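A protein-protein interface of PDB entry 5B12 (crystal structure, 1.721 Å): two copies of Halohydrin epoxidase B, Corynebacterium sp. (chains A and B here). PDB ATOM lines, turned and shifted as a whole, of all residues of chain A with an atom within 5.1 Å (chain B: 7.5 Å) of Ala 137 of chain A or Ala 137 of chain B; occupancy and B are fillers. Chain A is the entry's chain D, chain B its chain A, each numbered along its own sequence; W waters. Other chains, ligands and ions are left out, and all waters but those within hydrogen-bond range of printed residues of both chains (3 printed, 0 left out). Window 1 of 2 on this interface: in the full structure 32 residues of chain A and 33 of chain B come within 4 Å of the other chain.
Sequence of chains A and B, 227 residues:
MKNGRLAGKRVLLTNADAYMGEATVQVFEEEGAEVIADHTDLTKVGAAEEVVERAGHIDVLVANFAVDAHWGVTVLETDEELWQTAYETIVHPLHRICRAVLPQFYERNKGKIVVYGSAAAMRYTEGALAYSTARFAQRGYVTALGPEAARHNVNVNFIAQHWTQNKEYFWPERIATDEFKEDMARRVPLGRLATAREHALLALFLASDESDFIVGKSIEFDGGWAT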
ATOM      1  N   TYR A  87      22.127 -38.457 -19.389  1.00  0.00           N
ATOM      2  CA  TYR A  87      21.084 -37.903 -18.532  1.00  0.00           C
ATOM      3  C   TYR A  87      20.226 -39.007 -17.922  1.00  0.00           C
ATOM      4  O   TYR A  87      19.903 -38.966 -16.729  1.00  0.00           O
ATOM      5  CB  TYR A  87      20.227 -36.906 -19.329  1.00  0.00           C
ATOM      6  CG  TYR A  87      21.034 -35.653 -19.530  1.00  0.00           C
ATOM      7  CD1 TYR A  87      20.953 -34.604 -18.612  1.00  0.00           C
ATOM      8  CD2 TYR A  87      21.946 -35.564 -20.564  1.00  0.00           C
ATOM      9  CE1 TYR A  87      21.744 -33.470 -18.757  1.00  0.00           C
ATOM     10  CE2 TYR A  87      22.749 -34.438 -20.712  1.00  0.00           C
ATOM     11  CZ  TYR A  87      22.634 -33.397 -19.805  1.00  0.00           C
ATOM     12  OH  TYR A  87      23.428 -32.276 -19.953  1.00  0.00           O
ATOM     13  N   VAL A  91      21.400 -38.382 -14.238  1.00  0.00           N
ATOM     14  CA  VAL A  91      20.732 -37.117 -13.910  1.00  0.00           C
ATOM     15  C   VAL A  91      19.317 -37.363 -13.403  1.00  0.00           C
ATOM     16  O   VAL A  91      18.997 -37.058 -12.247  1.00  0.00           O
ATOM     17  CB  VAL A  91      20.719 -36.174 -15.125  1.00  0.00           C
ATOM     18  CG1 VAL A  91      19.974 -34.846 -14.771  1.00  0.00           C
ATOM     19  CG2 VAL A  91      22.144 -35.892 -15.586  1.00  0.00           C
ATOM     20  N   SER A 132      30.307 -34.702 -18.927  1.00  0.00           N
ATOM     21  CA  SER A 132      30.557 -33.483 -18.172  1.00  0.00           C
ATOM     22  C   SER A 132      29.268 -32.710 -17.936  1.00  0.00           C
ATOM     23  O   SER A 132      29.019 -32.241 -16.823  1.00  0.00           O
ATOM     24  CB  SER A 132      31.582 -32.627 -18.910  1.00  0.00           C
ATOM     25  OG  SER A 132      32.855 -33.248 -18.879  1.00  0.00           O
ATOM     26  N   THR A 133      28.429 -32.571 -18.969  1.00  0.00           N
ATOM     27  CA  THR A 133      27.206 -31.784 -18.783  1.00  0.00           C
ATOM     28  C   THR A 133      26.250 -32.480 -17.819  1.00  0.00           C
ATOM     29  O   THR A 133      25.558 -31.831 -17.033  1.00  0.00           O
ATOM     30  CB  THR A 133      26.521 -31.513 -20.121  1.00  0.00           C
ATOM     31  OG1 THR A 133      25.963 -32.726 -20.677  1.00  0.00           O
ATOM     32  CG2 THR A 133      27.528 -30.928 -21.125  1.00  0.00           C
ATOM     33  N   ALA A 134      26.195 -33.806 -17.870  1.00  0.00           N
ATOM     34  CA  ALA A 134      25.334 -34.536 -16.949  1.00  0.00           C
ATOM     35  C   ALA A 134      25.851 -34.448 -15.521  1.00  0.00           C
ATOM     36  O   ALA A 134      25.068 -34.291 -14.579  1.00  0.00           O
ATOM     37  CB  ALA A 134      25.206 -35.988 -17.432  1.00  0.00           C
ATOM     38  N   ARG A 135      27.170 -34.443 -15.335  1.00  0.00           N
ATOM     39  CA  ARG A 135      27.695 -34.220 -13.994  1.00  0.00           C
ATOM     40  C   ARG A 135      27.434 -32.791 -13.538  1.00  0.00           C
ATOM     41  O   ARG A 135      27.139 -32.567 -12.367  1.00  0.00           O
ATOM     42  CB  ARG A 135      29.183 -34.553 -13.939  1.00  0.00           C
ATOM     43  CG  ARG A 135      29.441 -36.084 -13.958  1.00  0.00           C
ATOM     44  CD  ARG A 135      29.033 -36.777 -12.652  1.00  0.00           C
ATOM     45  NE  ARG A 135      29.547 -38.157 -12.715  1.00  0.00           N
ATOM     46  CZ  ARG A 135      28.986 -39.216 -12.135  1.00  0.00           C
ATOM     47  NH1 ARG A 135      27.885 -39.090 -11.418  1.00  0.00           N
ATOM     48  NH2 ARG A 135      29.542 -40.414 -12.279  1.00  0.00           N
ATOM     49  N   PHE A 136      27.529 -31.815 -14.454  1.00  0.00           N
ATOM     50  CA  PHE A 136      27.112 -30.451 -14.127  1.00  0.00           C
ATOM     51  C   PHE A 136      25.670 -30.415 -13.637  1.00  0.00           C
ATOM     52  O   PHE A 136      25.351 -29.702 -12.678  1.00  0.00           O
ATOM     53  CB  PHE A 136      27.277 -29.522 -15.345  1.00  0.00           C
ATOM     54  CG  PHE A 136      28.489 -28.611 -15.277  1.00  0.00           C
ATOM     55  CD1 PHE A 136      29.705 -29.033 -15.772  1.00  0.00           C
ATOM     56  CD2 PHE A 136      28.381 -27.325 -14.774  1.00  0.00           C
ATOM     57  CE1 PHE A 136      30.810 -28.222 -15.743  1.00  0.00           C
ATOM     58  CE2 PHE A 136      29.504 -26.464 -14.753  1.00  0.00           C
ATOM     59  CZ  PHE A 136      30.721 -26.929 -15.231  1.00  0.00           C
ATOM     60  N   ALA A 137      24.775 -31.156 -14.289  1.00  0.00           N
ATOM     61  CA  ALA A 137      23.390 -31.163 -13.839  1.00  0.00           C
ATOM     62  C   ALA A 137      23.288 -31.714 -12.422  1.00  0.00           C
ATOM     63  O   ALA A 137      22.505 -31.216 -11.609  1.00  0.00           O
ATOM     64  CB  ALA A 137      22.539 -31.970 -14.829  1.00  0.00           C
ATOM     65  N   GLN A 138      24.109 -32.728 -12.089  1.00  0.00           N
ATOM     66  CA  GLN A 138      24.114 -33.251 -10.722  1.00  0.00           C
ATOM     67  C   GLN A 138      24.624 -32.230  -9.724  1.00  0.00           C
ATOM     68  O   GLN A 138      24.122 -32.147  -8.597  1.00  0.00           O
ATOM     69  CB  GLN A 138      24.998 -34.488 -10.609  1.00  0.00           C
ATOM     70  CG  GLN A 138      24.451 -35.728 -11.261  1.00  0.00           C
ATOM     71  CD  GLN A 138      25.278 -36.922 -10.842  1.00  0.00           C
ATOM     72  OE1 GLN A 138      26.496 -36.800 -10.653  1.00  0.00           O
ATOM     73  NE2 GLN A 138      24.625 -38.073 -10.644  1.00  0.00           N
ATOM     74  N   ARG A 139      25.692 -31.522 -10.086  1.00  0.00           N
ATOM     75  CA  ARG A 139      26.181 -30.446  -9.243  1.00  0.00           C
ATOM     76  C   ARG A 139      25.100 -29.391  -9.045  1.00  0.00           C
ATOM     77  O   ARG A 139      24.894 -28.886  -7.927  1.00  0.00           O
ATOM     78  CB  ARG A 139      27.410 -29.830  -9.907  1.00  0.00           C
ATOM     79  CG  ARG A 139      27.980 -28.656  -9.144  1.00  0.00           C
ATOM     80  CD  ARG A 139      29.007 -27.964 -10.013  1.00  0.00           C
ATOM     81  NE  ARG A 139      29.454 -26.707  -9.420  1.00  0.00           N
ATOM     82  CZ  ARG A 139      30.219 -25.824 -10.061  1.00  0.00           C
ATOM     83  NH1 ARG A 139      30.604 -26.073 -11.305  1.00  0.00           N
ATOM     84  NH2 ARG A 139      30.596 -24.693  -9.455  1.00  0.00           N
ATOM     85  N   GLY A 140      24.407 -29.055 -10.127  1.00  0.00           N
ATOM     86  CA  GLY A 140      23.280 -28.146 -10.025  1.00  0.00           C
ATOM     87  C   GLY A 140      22.213 -28.659  -9.086  1.00  0.00           C
ATOM     88  O   GLY A 140      21.633 -27.895  -8.316  1.00  0.00           O
ATOM     89  N   TYR A 141      21.947 -29.968  -9.129  1.00  0.00           N
ATOM     90  CA  TYR A 141      20.954 -30.529  -8.215  1.00  0.00           C
ATOM     91  C   TYR A 141      21.353 -30.315  -6.766  1.00  0.00           C
ATOM     92  O   TYR A 141      20.530 -29.935  -5.932  1.00  0.00           O
ATOM     93  CB  TYR A 141      20.755 -32.017  -8.519  1.00  0.00           C
ATOM     94  CG  TYR A 141      19.551 -32.565  -7.802  1.00  0.00           C
ATOM     95  CD1 TYR A 141      18.275 -32.335  -8.299  1.00  0.00           C
ATOM     96  CD2 TYR A 141      19.687 -33.279  -6.631  1.00  0.00           C
ATOM     97  CE1 TYR A 141      17.159 -32.815  -7.656  1.00  0.00           C
ATOM     98  CE2 TYR A 141      18.574 -33.755  -5.965  1.00  0.00           C
ATOM     99  CZ  TYR A 141      17.319 -33.520  -6.491  1.00  0.00           C
ATOM    100  OH  TYR A 141      16.209 -33.995  -5.844  1.00  0.00           O
ATOM    101  N   TRP B  83      10.123 -32.111 -14.177  1.00  0.00           N
ATOM    102  CA  TRP B  83      11.558 -32.343 -14.303  1.00  0.00           C
ATOM    103  C   TRP B  83      11.963 -32.581 -15.755  1.00  0.00           C
ATOM    104  O   TRP B  83      12.859 -31.911 -16.278  1.00  0.00           O
ATOM    105  CB  TRP B  83      11.953 -33.525 -13.415  1.00  0.00           C
ATOM    106  CG  TRP B  83      13.392 -33.902 -13.553  1.00  0.00           C
ATOM    107  CD1 TRP B  83      13.933 -34.794 -14.425  1.00  0.00           C
ATOM    108  CD2 TRP B  83      14.480 -33.377 -12.783  1.00  0.00           C
ATOM    109  NE1 TRP B  83      15.301 -34.865 -14.245  1.00  0.00           N
ATOM    110  CE2 TRP B  83      15.657 -34.009 -13.239  1.00  0.00           C
ATOM    111  CE3 TRP B  83      14.568 -32.450 -11.739  1.00  0.00           C
ATOM    112  CZ2 TRP B  83      16.910 -33.741 -12.692  1.00  0.00           C
ATOM    113  CZ3 TRP B  83      15.823 -32.177 -11.192  1.00  0.00           C
ATOM    114  CH2 TRP B  83      16.975 -32.811 -11.687  1.00  0.00           C
ATOM    115  N   TYR B  87      14.518 -30.368 -18.969  1.00  0.00           N
ATOM    116  CA  TYR B  87      15.602 -30.894 -19.799  1.00  0.00           C
ATOM    117  C   TYR B  87      15.230 -30.916 -21.271  1.00  0.00           C
ATOM    118  O   TYR B  87      16.045 -30.548 -22.130  1.00  0.00           O
ATOM    119  CB  TYR B  87      15.990 -32.284 -19.296  1.00  0.00           C
ATOM    120  CG  TYR B  87      16.780 -32.127 -18.040  1.00  0.00           C
ATOM    121  CD1 TYR B  87      16.144 -31.962 -16.807  1.00  0.00           C
ATOM    122  CD2 TYR B  87      18.161 -32.043 -18.089  1.00  0.00           C
ATOM    123  CE1 TYR B  87      16.869 -31.769 -15.656  1.00  0.00           C
ATOM    124  CE2 TYR B  87      18.894 -31.848 -16.941  1.00  0.00           C
ATOM    125  CZ  TYR B  87      18.253 -31.714 -15.736  1.00  0.00           C
ATOM    126  OH  TYR B  87      18.992 -31.533 -14.581  1.00  0.00           O
ATOM    127  N   ILE B  90      15.258 -26.907 -22.679  1.00  0.00           N
ATOM    128  CA  ILE B  90      16.454 -26.071 -22.763  1.00  0.00           C
ATOM    129  C   ILE B  90      17.766 -26.845 -22.738  1.00  0.00           C
ATOM    130  O   ILE B  90      18.811 -26.241 -23.022  1.00  0.00           O
ATOM    131  CB  ILE B  90      16.467 -24.990 -21.666  1.00  0.00           C
ATOM    132  CG1 ILE B  90      16.862 -25.603 -20.327  1.00  0.00           C
ATOM    133  CG2 ILE B  90      15.103 -24.274 -21.596  1.00  0.00           C
ATOM    134  CD1 ILE B  90      17.052 -24.585 -19.260  1.00  0.00           C
ATOM    135  N   VAL B  91      17.770 -28.154 -22.450  1.00  0.00           N
ATOM    136  CA  VAL B  91      19.047 -28.869 -22.371  1.00  0.00           C
ATOM    137  C   VAL B  91      19.325 -29.664 -23.650  1.00  0.00           C
ATOM    138  O   VAL B  91      20.304 -29.407 -24.365  1.00  0.00           O
ATOM    139  CB  VAL B  91      19.081 -29.777 -21.125  1.00  0.00           C
ATOM    140  CG1 VAL B  91      20.415 -30.582 -21.076  1.00  0.00           C
ATOM    141  CG2 VAL B  91      18.930 -28.949 -19.857  1.00  0.00           C
ATOM    142  N   HIS B  92      18.483 -30.646 -23.968  1.00  0.00           N
ATOM    143  CA  HIS B  92      18.772 -31.436 -25.162  1.00  0.00           C
ATOM    144  C   HIS B  92      18.796 -30.605 -26.442  1.00  0.00           C
ATOM    145  O   HIS B  92      19.652 -30.883 -27.305  1.00  0.00           O
ATOM    146  CB  HIS B  92      17.769 -32.589 -25.274  1.00  0.00           C
ATOM    147  CG  HIS B  92      17.624 -33.361 -24.009  1.00  0.00           C
ATOM    148  ND1 HIS B  92      18.695 -33.650 -23.191  1.00  0.00           N
ATOM    149  CD2 HIS B  92      16.533 -33.889 -23.403  1.00  0.00           C
ATOM    150  CE1 HIS B  92      18.272 -34.324 -22.137  1.00  0.00           C
ATOM    151  NE2 HIS B  92      16.964 -34.484 -22.245  1.00  0.00           N
ATOM    152  N   LEU B  94      19.913 -27.688 -26.873  1.00  0.00           N
ATOM    153  CA  LEU B  94      21.154 -26.927 -26.932  1.00  0.00           C
ATOM    154  C   LEU B  94      22.237 -27.726 -27.647  1.00  0.00           C
ATOM    155  O   LEU B  94      22.923 -27.217 -28.541  1.00  0.00           O
ATOM    156  CB  LEU B  94      21.589 -26.533 -25.514  1.00  0.00           C
ATOM    157  CG  LEU B  94      22.904 -25.748 -25.403  1.00  0.00           C
ATOM    158  CD1 LEU B  94      22.783 -24.442 -26.215  1.00  0.00           C
ATOM    159  CD2 LEU B  94      23.276 -25.439 -23.968  1.00  0.00           C
ATOM    160  N   ALA B 121      22.242 -21.180 -12.919  1.00  0.00           N
ATOM    161  CA  ALA B 121      23.310 -22.125 -13.214  1.00  0.00           C
ATOM    162  C   ALA B 121      24.556 -21.859 -12.387  1.00  0.00           C
ATOM    163  O   ALA B 121      25.527 -22.600 -12.508  1.00  0.00           O
ATOM    164  CB  ALA B 121      23.663 -22.072 -14.707  1.00  0.00           C
ATOM    165  N   LEU B 129      13.967 -25.522  -8.645  1.00  0.00           N
ATOM    166  CA  LEU B 129      14.894 -26.652  -8.602  1.00  0.00           C
ATOM    167  C   LEU B 129      15.172 -27.225  -9.990  1.00  0.00           C
ATOM    168  O   LEU B 129      16.324 -27.265 -10.433  1.00  0.00           O
ATOM    169  CB  LEU B 129      14.352 -27.743  -7.671  1.00  0.00           C
ATOM    170  CG  LEU B 129      15.148 -29.050  -7.777  1.00  0.00           C
ATOM    171  CD1 LEU B 129      16.425 -28.896  -6.987  1.00  0.00           C
ATOM    172  CD2 LEU B 129      14.321 -30.215  -7.253  1.00  0.00           C
ATOM    173  N   TYR B 131      14.524 -26.210 -13.001  1.00  0.00           N
ATOM    174  CA  TYR B 131      15.046 -25.172 -13.877  1.00  0.00           C
ATOM    175  C   TYR B 131      16.516 -24.905 -13.587  1.00  0.00           C
ATOM    176  O   TYR B 131      17.335 -24.769 -14.511  1.00  0.00           O
ATOM    177  CB  TYR B 131      14.208 -23.912 -13.676  1.00  0.00           C
ATOM    178  CG  TYR B 131      14.736 -22.730 -14.446  1.00  0.00           C
ATOM    179  CD1 TYR B 131      14.641 -22.698 -15.816  1.00  0.00           C
ATOM    180  CD2 TYR B 131      15.354 -21.667 -13.794  1.00  0.00           C
ATOM    181  CE1 TYR B 131      15.127 -21.629 -16.533  1.00  0.00           C
ATOM    182  CE2 TYR B 131      15.840 -20.584 -14.512  1.00  0.00           C
ATOM    183  CZ  TYR B 131      15.723 -20.586 -15.877  1.00  0.00           C
ATOM    184  OH  TYR B 131      16.198 -19.534 -16.630  1.00  0.00           O
ATOM    185  N   SER B 132      16.859 -24.789 -12.307  1.00  0.00           N
ATOM    186  CA  SER B 132      18.249 -24.538 -11.940  1.00  0.00           C
ATOM    187  C   SER B 132      19.152 -25.641 -12.452  1.00  0.00           C
ATOM    188  O   SER B 132      20.232 -25.372 -12.991  1.00  0.00           O
ATOM    189  CB  SER B 132      18.392 -24.423 -10.428  1.00  0.00           C
ATOM    190  OG  SER B 132      17.724 -23.265  -9.956  1.00  0.00           O
ATOM    191  N   THR B 133      18.730 -26.897 -12.297  1.00  0.00           N
ATOM    192  CA  THR B 133      19.612 -27.981 -12.718  1.00  0.00           C
ATOM    193  C   THR B 133      19.747 -28.018 -14.231  1.00  0.00           C
ATOM    194  O   THR B 133      20.832 -28.306 -14.747  1.00  0.00           O
ATOM    195  CB  THR B 133      19.101 -29.325 -12.185  1.00  0.00           C
ATOM    196  OG1 THR B 133      17.880 -29.669 -12.842  1.00  0.00           O
ATOM    197  CG2 THR B 133      18.866 -29.248 -10.696  1.00  0.00           C
ATOM    198  N   ALA B 134      18.693 -27.643 -14.955  1.00  0.00           N
ATOM    199  CA  ALA B 134      18.776 -27.601 -16.407  1.00  0.00           C
ATOM    200  C   ALA B 134      19.686 -26.472 -16.874  1.00  0.00           C
ATOM    201  O   ALA B 134      20.461 -26.633 -17.830  1.00  0.00           O
ATOM    202  CB  ALA B 134      17.375 -27.452 -16.994  1.00  0.00           C
ATOM    203  N   ARG B 135      19.622 -25.327 -16.205  1.00  0.00           N
ATOM    204  CA  ARG B 135      20.563 -24.269 -16.544  1.00  0.00           C
ATOM    205  C   ARG B 135      21.993 -24.652 -16.168  1.00  0.00           C
ATOM    206  O   ARG B 135      22.932 -24.325 -16.904  1.00  0.00           O
ATOM    207  CB  ARG B 135      20.138 -22.972 -15.878  1.00  0.00           C
ATOM    208  CG  ARG B 135      18.863 -22.367 -16.513  1.00  0.00           C
ATOM    209  CD  ARG B 135      19.098 -21.768 -17.901  1.00  0.00           C
ATOM    210  NE  ARG B 135      17.929 -20.977 -18.312  1.00  0.00           N
ATOM    211  CZ  ARG B 135      17.526 -20.761 -19.565  1.00  0.00           C
ATOM    212  NH1 ARG B 135      18.184 -21.263 -20.605  1.00  0.00           N
ATOM    213  NH2 ARG B 135      16.424 -20.044 -19.774  1.00  0.00           N
ATOM    214  N   PHE B 136      22.190 -25.345 -15.040  1.00  0.00           N
ATOM    215  CA  PHE B 136      23.516 -25.899 -14.751  1.00  0.00           C
ATOM    216  C   PHE B 136      23.999 -26.798 -15.875  1.00  0.00           C
ATOM    217  O   PHE B 136      25.183 -26.798 -16.208  1.00  0.00           O
ATOM    218  CB  PHE B 136      23.498 -26.701 -13.447  1.00  0.00           C
ATOM    219  CG  PHE B 136      24.099 -25.988 -12.280  1.00  0.00           C
ATOM    220  CD1 PHE B 136      23.307 -25.168 -11.490  1.00  0.00           C
ATOM    221  CD2 PHE B 136      25.437 -26.156 -11.953  1.00  0.00           C
ATOM    222  CE1 PHE B 136      23.831 -24.522 -10.395  1.00  0.00           C
ATOM    223  CE2 PHE B 136      25.973 -25.532 -10.854  1.00  0.00           C
ATOM    224  CZ  PHE B 136      25.166 -24.698 -10.067  1.00  0.00           C
ATOM    225  N   ALA B 137      23.106 -27.611 -16.451  1.00  0.00           N
ATOM    226  CA  ALA B 137      23.536 -28.463 -17.549  1.00  0.00           C
ATOM    227  C   ALA B 137      23.948 -27.630 -18.755  1.00  0.00           C
ATOM    228  O   ALA B 137      24.901 -27.981 -19.455  1.00  0.00           O
ATOM    229  CB  ALA B 137      22.431 -29.450 -17.928  1.00  0.00           C
ATOM    230  N   GLN B 138      23.252 -26.521 -19.007  1.00  0.00           N
ATOM    231  CA  GLN B 138      23.651 -25.649 -20.106  1.00  0.00           C
ATOM    232  C   GLN B 138      25.001 -25.035 -19.834  1.00  0.00           C
ATOM    233  O   GLN B 138      25.839 -24.922 -20.735  1.00  0.00           O
ATOM    234  CB  GLN B 138      22.647 -24.523 -20.299  1.00  0.00           C
ATOM    235  CG  GLN B 138      21.314 -24.913 -20.903  1.00  0.00           C
ATOM    236  CD  GLN B 138      20.596 -23.675 -21.335  1.00  0.00           C
ATOM    237  OE1 GLN B 138      20.664 -22.648 -20.646  1.00  0.00           O
ATOM    238  NE2 GLN B 138      19.950 -23.723 -22.485  1.00  0.00           N
ATOM    239  N   ARG B 139      25.199 -24.571 -18.603  1.00  0.00           N
ATOM    240  CA  ARG B 139      26.500 -24.042 -18.243  1.00  0.00           C
ATOM    241  C   ARG B 139      27.570 -25.090 -18.457  1.00  0.00           C
ATOM    242  O   ARG B 139      28.653 -24.796 -18.968  1.00  0.00           O
ATOM    243  CB  ARG B 139      26.477 -23.592 -16.792  1.00  0.00           C
ATOM    244  CG  ARG B 139      27.836 -23.239 -16.256  1.00  0.00           C
ATOM    245  CD  ARG B 139      27.715 -22.990 -14.786  1.00  0.00           C
ATOM    246  NE  ARG B 139      28.983 -22.573 -14.212  1.00  0.00           N
ATOM    247  CZ  ARG B 139      29.248 -22.535 -12.912  1.00  0.00           C
ATOM    248  NH1 ARG B 139      28.333 -22.880 -12.013  1.00  0.00           N
ATOM    249  NH2 ARG B 139      30.443 -22.128 -12.512  1.00  0.00           N
ATOM    250  N   GLY B 140      27.277 -26.334 -18.087  1.00  0.00           N
ATOM    251  CA  GLY B 140      28.246 -27.387 -18.313  1.00  0.00           C
ATOM    252  C   GLY B 140      28.537 -27.589 -19.777  1.00  0.00           C
ATOM    253  O   GLY B 140      29.681 -27.859 -20.159  1.00  0.00           O
ATOM    254  N   TYR B 141      27.503 -27.473 -20.620  1.00  0.00           N
ATOM    255  CA  TYR B 141      27.689 -27.582 -22.059  1.00  0.00           C
ATOM    256  C   TYR B 141      28.701 -26.560 -22.569  1.00  0.00           C
ATOM    257  O   TYR B 141      29.585 -26.891 -23.372  1.00  0.00           O
ATOM    258  CB  TYR B 141      26.342 -27.405 -22.775  1.00  0.00           C
ATOM    259  CG  TYR B 141      26.447 -27.819 -24.217  1.00  0.00           C
ATOM    260  CD1 TYR B 141      26.480 -29.165 -24.555  1.00  0.00           C
ATOM    261  CD2 TYR B 141      26.557 -26.883 -25.234  1.00  0.00           C
ATOM    262  CE1 TYR B 141      26.615 -29.567 -25.867  1.00  0.00           C
ATOM    263  CE2 TYR B 141      26.685 -27.280 -26.567  1.00  0.00           C
ATOM    264  CZ  TYR B 141      26.719 -28.625 -26.865  1.00  0.00           C
ATOM    265  OH  TYR B 141      26.859 -29.040 -28.168  1.00  0.00           O
ATOM    266  N   VAL B 142      28.585 -25.311 -22.110  1.00  0.00           N
ATOM    267  CA  VAL B 142      29.525 -24.273 -22.526  1.00  0.00           C
ATOM    268  C   VAL B 142      30.913 -24.541 -21.946  1.00  0.00           C
ATOM    269  O   VAL B 142      31.932 -24.373 -22.633  1.00  0.00           O
ATOM    270  CB  VAL B 142      28.973 -22.898 -22.114  1.00  0.00           C
ATOM    271  CG1 VAL B 142      30.054 -21.822 -22.250  1.00  0.00           C
ATOM    272  CG2 VAL B 142      27.724 -22.578 -22.933  1.00  0.00           C
ATOM    273  N   THR B 143      30.978 -24.985 -20.686  1.00  0.00           N
ATOM    274  CA  THR B 143      32.265 -25.283 -20.060  1.00  0.00           C
ATOM    275  C   THR B 143      32.983 -26.419 -20.770  1.00  0.00           C
ATOM    276  O   THR B 143      34.219 -26.402 -20.898  1.00  0.00           O
ATOM    277  CB  THR B 143      32.048 -25.638 -18.591  1.00  0.00           C
ATOM    278  OG1 THR B 143      31.418 -24.525 -17.941  1.00  0.00           O
ATOM    279  CG2 THR B 143      33.392 -25.974 -17.885  1.00  0.00           C
ATOM    280  N   PHE B 158      28.538 -18.344 -22.286  1.00  0.00           N
ATOM    281  CA  PHE B 158      27.282 -18.511 -21.567  1.00  0.00           C
ATOM    282  C   PHE B 158      26.959 -17.217 -20.839  1.00  0.00           C
ATOM    283  O   PHE B 158      27.775 -16.751 -20.044  1.00  0.00           O
ATOM    284  CB  PHE B 158      27.455 -19.667 -20.582  1.00  0.00           C
ATOM    285  CG  PHE B 158      26.236 -20.014 -19.751  1.00  0.00           C
ATOM    286  CD1 PHE B 158      25.274 -20.886 -20.242  1.00  0.00           C
ATOM    287  CD2 PHE B 158      26.142 -19.596 -18.430  1.00  0.00           C
ATOM    288  CE1 PHE B 158      24.202 -21.289 -19.440  1.00  0.00           C
ATOM    289  CE2 PHE B 158      25.072 -19.984 -17.617  1.00  0.00           C
ATOM    290  CZ  PHE B 158      24.087 -20.839 -18.144  1.00  0.00           C
HETATM  291  O   HOH W   1      32.700 -23.320 -10.585  1.00  0.00           O
HETATM  292  O   HOH W   2      31.041 -21.737  -9.428  1.00  0.00           O
HETATM  293  O   HOH W   3      32.388 -24.433 -12.909  1.00  0.00           O
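Tyr 87 of chain A touches Ala 137 of chain B, and with the chains exchanged Ala 137 of chain A touches Tyr 87 of chain B.
Thr 133 of chain A touches Tyr 141 of chain B, and with the chains exchanged Tyr 141 of chain A touches Thr 133 of chain B.
Phe 136 of chain A touches Arg 139 of chain B, and with the chains exchanged Arg 139 of chain A touches Phe 136 of chain B.
Arg 139 of chain A touches its own counterpart, Arg 139 of chain B.
Of the 22 pairs that touch across the chains among the printed residues, 18 have their exchanged pair printed and touching as well.
CE2 of Tyr 87 of chain B touches CE1 of Tyr 87 of chain A, at 3.7 Å.
Ala 137 of chain B touches Tyr 87 of chain A.
Val 91 of chain A touches Trp 83 of chain B.
Tyr 87 of chain B touches Val 91 of chain A.
Thr 133 of chain A touches Gly 140 of chain B.
Phe 136 of chain A touches Thr 143 of chain B.
Tyr 87 of chain B touches Ala 137 of chain A (OH to CB, 3.6 Å).
Thr 133 of chain B touches Ala 137 of chain A.
NE of Arg 139 of chain A touches CE2 of Phe 136 of chain B, 3.9 Å away.
Trp 83 of chain B touches Tyr 141 of chain A (CH2 to CD1, 3.7 Å).
Of the printed residues of chain B, Ala 137 of chain A touches Tyr 87 (3.6 Å), Thr 133 (3.9 Å) and Ala 137 (3.996 Å).
Of the printed residues of chain A, Ala 137 of chain B touches Tyr 87, Thr 133 and Ala 137.
Of the printed residues of chain A, Gly 140 of chain B touches Thr 133 and Phe 136.
Printed residues of chain A within 4 Å of Thr 143 of chain B: Phe 136 (3.7 Å).
The nearest printed residue of chain B that does not touch Ala 137 of chain A is Phe 136 of chain B (4.5 Å).
Printed residues of chain B that touch a printed residue of chain A: Trp 83, Tyr 87, Val 91, Leu 129, Thr 133, Phe 136, Ala 137, Arg 139, Gly 140, Tyr 141 and Thr 143.
Along chain B the printed residues that touch a printed residue of chain A span positions 83 to 143.
Of the 12 printed residues of chain A, 8 touch a printed residue of chain B.
Among the printed residues, no Asp or Glu carboxylate lies within 4 Å of a Lys or Arg side-chain nitrogen of the other chain.
Water W1 bridges NH2 of Arg 139 of chain A (2.8 Å) and NH2 of Arg 139 of chain B (3.2 Å).
Water W3 bridges the guanidinium group of Arg 139 of chain A (2.9 Å) and the guanidinium group of Arg 139 of chain B (3.0 Å).
Water W2 bridges NH2 of Arg 139 of chain A and NH2 of Arg 139 of chain B.
OG1 of Thr 133 of chain B lies within hydrogen-bond range of OH of Tyr 87 of chain B, at 2.8 Å.
The backbone carbonyl oxygen of Ala 121 of chain B sits at hydrogen-bond distance from the guanidinium group of Arg 139 of chain B, at 2.9 Å.
The backbone carbonyl oxygen of Arg 139 of chain B sits at hydrogen-bond distance from the side-chain hydroxyl of Thr 143 of chain B (3.0 Å).
The side-chain hydroxyl (OG1) of Thr 133 of chain A lies within hydrogen-bond range of the side-chain hydroxyl (OH) of Tyr 87 of chain A (2.7 Å).
O of Tyr 87 of chain B lies within hydrogen-bond range of N of His 92 of chain B, at 3.1 Å.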
